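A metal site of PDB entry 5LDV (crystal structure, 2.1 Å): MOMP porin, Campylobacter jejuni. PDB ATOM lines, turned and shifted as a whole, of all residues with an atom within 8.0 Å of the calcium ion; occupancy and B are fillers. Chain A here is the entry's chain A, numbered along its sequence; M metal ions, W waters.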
ATOM      1  N   ARG A  48     -12.086  33.554   5.722  1.00  0.00           N
ATOM      2  CA  ARG A  48     -11.297  32.446   5.163  1.00  0.00           C
ATOM      3  C   ARG A  48     -12.161  31.846   4.070  1.00  0.00           C
ATOM      4  O   ARG A  48     -13.336  31.508   4.319  1.00  0.00           O
ATOM      5  CB  ARG A  48     -11.005  31.405   6.236  1.00  0.00           C
ATOM      6  CG  ARG A  48     -10.046  30.287   5.792  1.00  0.00           C
ATOM      7  CD  ARG A  48      -8.693  30.875   5.532  1.00  0.00           C
ATOM      8  NE  ARG A  48      -7.682  29.901   5.147  1.00  0.00           N
ATOM      9  CZ  ARG A  48      -6.955  29.191   5.993  1.00  0.00           C
ATOM     10  NH1 ARG A  48      -7.121  29.320   7.308  1.00  0.00           N
ATOM     11  NH2 ARG A  48      -6.047  28.347   5.528  1.00  0.00           N
ATOM     12  N   ARG A  91      -2.899  26.909  -2.759  1.00  0.00           N
ATOM     13  CA  ARG A  91      -2.597  26.271  -1.501  1.00  0.00           C
ATOM     14  C   ARG A  91      -2.367  24.767  -1.658  1.00  0.00           C
ATOM     15  O   ARG A  91      -1.629  24.172  -0.848  1.00  0.00           O
ATOM     16  CB  ARG A  91      -3.756  26.536  -0.542  1.00  0.00           C
ATOM     17  CG  ARG A  91      -3.592  25.981   0.844  1.00  0.00           C
ATOM     18  CD  ARG A  91      -4.585  26.616   1.828  1.00  0.00           C
ATOM     19  NE  ARG A  91      -4.194  26.284   3.192  1.00  0.00           N
ATOM     20  CZ  ARG A  91      -4.464  25.134   3.795  1.00  0.00           C
ATOM     21  NH1 ARG A  91      -5.217  24.213   3.198  1.00  0.00           N
ATOM     22  NH2 ARG A  91      -4.005  24.913   5.009  1.00  0.00           N
ATOM     23  N   THR A 118      -2.184  16.235  12.364  1.00  0.00           N
ATOM     24  CA  THR A 118      -2.444  17.565  11.778  1.00  0.00           C
ATOM     25  C   THR A 118      -3.924  17.840  11.705  1.00  0.00           C
ATOM     26  O   THR A 118      -4.761  16.916  11.709  1.00  0.00           O
ATOM     27  CB  THR A 118      -1.832  17.715  10.371  1.00  0.00           C
ATOM     28  OG1 THR A 118      -2.481  16.824   9.431  1.00  0.00           O
ATOM     29  CG2 THR A 118      -0.365  17.449  10.373  1.00  0.00           C
ATOM     30  N   ASP A 119      -4.269  19.117  11.599  1.00  0.00           N
ATOM     31  CA  ASP A 119      -5.658  19.523  11.449  1.00  0.00           C
ATOM     32  C   ASP A 119      -6.131  19.053  10.089  1.00  0.00           C
ATOM     33  O   ASP A 119      -5.413  19.212   9.117  1.00  0.00           O
ATOM     34  CB  ASP A 119      -5.724  21.034  11.587  1.00  0.00           C
ATOM     35  CG  ASP A 119      -7.127  21.606  11.476  1.00  0.00           C
ATOM     36  OD1 ASP A 119      -8.141  20.879  11.334  1.00  0.00           O
ATOM     37  OD2 ASP A 119      -7.195  22.845  11.464  1.00  0.00           O
ATOM     38  N   ASN A 120      -7.296  18.415  10.026  1.00  0.00           N
ATOM     39  CA  ASN A 120      -7.839  17.917   8.784  1.00  0.00           C
ATOM     40  C   ASN A 120      -8.900  18.873   8.209  1.00  0.00           C
ATOM     41  O   ASN A 120      -9.559  18.542   7.236  1.00  0.00           O
ATOM     42  CB  ASN A 120      -8.470  16.540   8.998  1.00  0.00           C
ATOM     43  CG  ASN A 120      -7.439  15.430   9.190  1.00  0.00           C
ATOM     44  OD1 ASN A 120      -6.400  15.604   9.863  1.00  0.00           O
ATOM     45  ND2 ASN A 120      -7.704  14.326   8.582  1.00  0.00           N
ATOM     46  N   GLY A 121      -9.086  20.028   8.847  1.00  0.00           N
ATOM     47  CA  GLY A 121     -10.094  20.994   8.411  1.00  0.00           C
ATOM     48  C   GLY A 121      -9.528  22.023   7.439  1.00  0.00           C
ATOM     49  O   GLY A 121      -8.543  21.765   6.692  1.00  0.00           O
ATOM     50  N   VAL A 122     -10.136  23.201   7.449  1.00  0.00           N
ATOM     51  CA  VAL A 122      -9.781  24.294   6.568  1.00  0.00           C
ATOM     52  C   VAL A 122      -8.302  24.665   6.642  1.00  0.00           C
ATOM     53  O   VAL A 122      -7.661  24.909   5.632  1.00  0.00           O
ATOM     54  CB  VAL A 122     -10.587  25.571   6.937  1.00  0.00           C
ATOM     55  CG1 VAL A 122     -10.132  26.748   6.070  1.00  0.00           C
ATOM     56  CG2 VAL A 122     -12.074  25.323   6.720  1.00  0.00           C
ATOM     57  N   ASP A 123      -7.784  24.751   7.859  1.00  0.00           N
ATOM     58  CA  ASP A 123      -6.451  25.268   8.078  1.00  0.00           C
ATOM     59  C   ASP A 123      -5.432  24.155   8.356  1.00  0.00           C
ATOM     60  O   ASP A 123      -4.488  24.359   9.112  1.00  0.00           O
ATOM     61  CB  ASP A 123      -6.472  26.249   9.240  1.00  0.00           C
ATOM     62  CG  ASP A 123      -5.251  27.133   9.284  1.00  0.00           C
ATOM     63  OD1 ASP A 123      -4.911  27.738   8.221  1.00  0.00           O
ATOM     64  OD2 ASP A 123      -4.642  27.215  10.357  1.00  0.00           O
ATOM     65  N   GLY A 124      -5.575  22.999   7.724  1.00  0.00           N
ATOM     66  CA  GLY A 124      -4.616  21.902   7.936  1.00  0.00           C
ATOM     67  C   GLY A 124      -3.250  22.106   7.268  1.00  0.00           C
ATOM     68  O   GLY A 124      -3.115  22.704   6.184  1.00  0.00           O
ATOM     69  N   LEU A 125      -2.237  21.584   7.924  1.00  0.00           N
ATOM     70  CA  LEU A 125      -0.893  21.600   7.399  1.00  0.00           C
ATOM     71  C   LEU A 125      -0.827  21.041   5.988  1.00  0.00           C
ATOM     72  O   LEU A 125      -1.363  19.958   5.714  1.00  0.00           O
ATOM     73  CB  LEU A 125       0.010  20.780   8.317  1.00  0.00           C
ATOM     74  CG  LEU A 125       1.467  20.751   7.905  1.00  0.00           C
ATOM     75  CD1 LEU A 125       1.986  22.163   7.713  1.00  0.00           C
ATOM     76  CD2 LEU A 125       2.266  19.965   8.938  1.00  0.00           C
ATOM     77  N   VAL A 126      -0.162  21.772   5.106  1.00  0.00           N
ATOM     78  CA  VAL A 126       0.090  21.334   3.746  1.00  0.00           C
ATOM     79  C   VAL A 126       1.563  20.989   3.599  1.00  0.00           C
ATOM     80  O   VAL A 126       2.447  21.626   4.202  1.00  0.00           O
ATOM     81  CB  VAL A 126      -0.318  22.473   2.771  1.00  0.00           C
ATOM     82  CG1 VAL A 126       0.091  22.194   1.350  1.00  0.00           C
ATOM     83  CG2 VAL A 126      -1.823  22.686   2.837  1.00  0.00           C
ATOM     84  N   GLU A 154       2.597  29.456   6.439  1.00  0.00           N
ATOM     85  CA  GLU A 154       1.168  29.715   6.530  1.00  0.00           C
ATOM     86  C   GLU A 154       0.645  29.350   7.925  1.00  0.00           C
ATOM     87  O   GLU A 154      -0.264  29.979   8.420  1.00  0.00           O
ATOM     88  CB  GLU A 154       0.395  28.884   5.501  1.00  0.00           C
ATOM     89  CG  GLU A 154      -1.127  29.101   5.549  1.00  0.00           C
ATOM     90  CD  GLU A 154      -1.964  27.935   5.017  1.00  0.00           C
ATOM     91  OE1 GLU A 154      -1.640  26.722   5.203  1.00  0.00           O
ATOM     92  OE2 GLU A 154      -2.970  28.247   4.396  1.00  0.00           O
ATOM     93  N   GLN A 155       1.195  28.325   8.544  1.00  0.00           N
ATOM     94  CA  GLN A 155       0.687  27.836   9.836  1.00  0.00           C
ATOM     95  C   GLN A 155       1.113  28.640  11.051  1.00  0.00           C
ATOM     96  O   GLN A 155       0.481  28.553  12.071  1.00  0.00           O
ATOM     97  CB  GLN A 155       1.137  26.382  10.018  1.00  0.00           C
ATOM     98  CG  GLN A 155       0.448  25.447   9.035  1.00  0.00           C
ATOM     99  CD  GLN A 155      -1.053  25.467   9.208  1.00  0.00           C
ATOM    100  OE1 GLN A 155      -1.588  25.419  10.352  1.00  0.00           O
ATOM    101  NE2 GLN A 155      -1.767  25.559   8.104  1.00  0.00           N
ATOM    102  N   GLY A 156       2.186  29.422  10.941  1.00  0.00           N
ATOM    103  CA  GLY A 156       2.761  30.159  12.082  1.00  0.00           C
ATOM    104  C   GLY A 156       2.840  29.304  13.330  1.00  0.00           C
ATOM    105  O   GLY A 156       3.343  28.169  13.301  1.00  0.00           O
ATOM    106  N   SER A 157       2.248  29.801  14.405  1.00  0.00           N
ATOM    107  CA  SER A 157       2.328  29.154  15.713  1.00  0.00           C
ATOM    108  C   SER A 157       1.576  27.827  15.846  1.00  0.00           C
ATOM    109  O   SER A 157       1.732  27.142  16.855  1.00  0.00           O
ATOM    110  CB  SER A 157       1.926  30.129  16.825  1.00  0.00           C
ATOM    111  OG  SER A 157       0.574  30.533  16.701  1.00  0.00           O
ATOM    112  N   ASP A 158       0.778  27.424  14.846  1.00  0.00           N
ATOM    113  CA  ASP A 158       0.171  26.089  14.856  1.00  0.00           C
ATOM    114  C   ASP A 158       1.204  24.969  14.716  1.00  0.00           C
ATOM    115  O   ASP A 158       0.996  23.852  15.231  1.00  0.00           O
ATOM    116  CB  ASP A 158      -0.816  25.935  13.700  1.00  0.00           C
ATOM    117  CG  ASP A 158      -2.125  26.607  13.959  1.00  0.00           C
ATOM    118  OD1 ASP A 158      -2.221  27.281  14.997  1.00  0.00           O
ATOM    119  OD2 ASP A 158      -3.078  26.413  13.145  1.00  0.00           O
ATOM    120  N   LEU A 159       2.314  25.241  14.041  1.00  0.00           N
ATOM    121  CA  LEU A 159       3.295  24.204  13.782  1.00  0.00           C
ATOM    122  C   LEU A 159       4.270  23.999  14.926  1.00  0.00           C
ATOM    123  O   LEU A 159       4.821  24.964  15.474  1.00  0.00           O
ATOM    124  CB  LEU A 159       4.046  24.467  12.472  1.00  0.00           C
ATOM    125  CG  LEU A 159       5.029  23.416  11.948  1.00  0.00           C
ATOM    126  CD1 LEU A 159       4.376  22.090  11.622  1.00  0.00           C
ATOM    127  CD2 LEU A 159       5.713  23.941  10.675  1.00  0.00           C
ATOM    128  N   GLU A 291       0.792  19.706  14.185  1.00  0.00           N
ATOM    129  CA  GLU A 291       0.164  21.013  13.878  1.00  0.00           C
ATOM    130  C   GLU A 291      -1.168  21.249  14.595  1.00  0.00           C
ATOM    131  O   GLU A 291      -2.084  20.438  14.477  1.00  0.00           O
ATOM    132  CB  GLU A 291       0.017  21.153  12.360  1.00  0.00           C
ATOM    133  CG  GLU A 291      -0.656  22.430  11.921  1.00  0.00           C
ATOM    134  CD  GLU A 291      -2.088  22.209  11.485  1.00  0.00           C
ATOM    135  OE1 GLU A 291      -2.405  21.157  10.872  1.00  0.00           O
ATOM    136  OE2 GLU A 291      -2.903  23.099  11.778  1.00  0.00           O
ATOM    137  N   ASP A 292      -1.253  22.352  15.327  1.00  0.00           N
ATOM    138  CA  ASP A 292      -2.454  22.820  16.063  1.00  0.00           C
ATOM    139  C   ASP A 292      -2.933  21.791  17.107  1.00  0.00           C
ATOM    140  O   ASP A 292      -2.301  21.666  18.142  1.00  0.00           O
ATOM    141  CB  ASP A 292      -3.579  23.261  15.094  1.00  0.00           C
ATOM    142  CG  ASP A 292      -4.716  24.029  15.788  1.00  0.00           C
ATOM    143  OD1 ASP A 292      -4.631  24.282  17.024  1.00  0.00           O
ATOM    144  OD2 ASP A 292      -5.696  24.363  15.083  1.00  0.00           O
ATOM    145  N   GLN A 293      -4.036  21.088  16.855  1.00  0.00           N
ATOM    146  CA  GLN A 293      -4.550  20.047  17.777  1.00  0.00           C
ATOM    147  C   GLN A 293      -4.695  18.718  17.075  1.00  0.00           C
ATOM    148  O   GLN A 293      -5.357  17.807  17.568  1.00  0.00           O
ATOM    149  CB  GLN A 293      -5.881  20.500  18.419  1.00  0.00           C
ATOM    150  CG  GLN A 293      -5.645  21.666  19.378  1.00  0.00           C
ATOM    151  CD  GLN A 293      -6.913  22.242  19.997  1.00  0.00           C
ATOM    152  OE1 GLN A 293      -7.993  22.126  19.463  1.00  0.00           O
ATOM    153  NE2 GLN A 293      -6.753  22.903  21.118  1.00  0.00           N
ATOM    154  N   TYR A 307      -5.138  25.765  24.816  1.00  0.00           N
ATOM    155  CA  TYR A 307      -4.148  26.690  24.309  1.00  0.00           C
ATOM    156  C   TYR A 307      -3.341  27.408  25.406  1.00  0.00           C
ATOM    157  O   TYR A 307      -2.407  28.154  25.111  1.00  0.00           O
ATOM    158  CB  TYR A 307      -4.782  27.700  23.353  1.00  0.00           C
ATOM    159  CG  TYR A 307      -5.234  27.063  22.047  1.00  0.00           C
ATOM    160  CD1 TYR A 307      -4.345  26.303  21.261  1.00  0.00           C
ATOM    161  CD2 TYR A 307      -6.529  27.221  21.593  1.00  0.00           C
ATOM    162  CE1 TYR A 307      -4.741  25.715  20.075  1.00  0.00           C
ATOM    163  CE2 TYR A 307      -6.964  26.645  20.394  1.00  0.00           C
ATOM    164  CZ  TYR A 307      -6.070  25.909  19.641  1.00  0.00           C
ATOM    165  OH  TYR A 307      -6.481  25.344  18.480  1.00  0.00           O
HETATM  166 CA    CA M   1      -3.648  25.230  11.264  1.00  0.00          CA
HETATM  167  O   HOH W   1      -5.516  24.661  12.552  1.00  0.00           O
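NE2 of Gln 155 lies within hydrogen-bond range of OE1 of Glu 154, 3.1 Å away.
O of Asp 158 sits at hydrogen-bond distance from N of Asp 292 (2.7 Å).
OE1 of Glu 291 is in hydrogen-bond range of N of Asp 119 (2.9 Å).
OE1 of Glu 291 is in hydrogen-bond range of N of Leu 125.
The side-chain carboxylate (OD1) of Asp 123 is in salt-bridge range of the guanidinium group (NH1) of Arg 48, at 2.9 Å.
Of the 21 residues printed, 4 come within 4 Å of the calcium ion.
Along chain A the residues within 4 Å of the calcium ion span positions 123 to 291.
The calcium ion is bound by OE1 of Gln 155 (2.3 Å), OD2 of Asp 158 (2.3 Å), OE2 of Glu 291 (2.3 Å), water W1 (2.3 Å), OD2 of Asp 123 (2.4 Å) and O of Asp 123 (2.5 Å).
The calcium ion has six donor atoms within binding distance.
Water W1 lies within hydrogen-bond range of the side-chain carboxylate of Asp 292 (2.6 Å) and the side-chain carboxylate of Asp 119 (2.7 Å).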
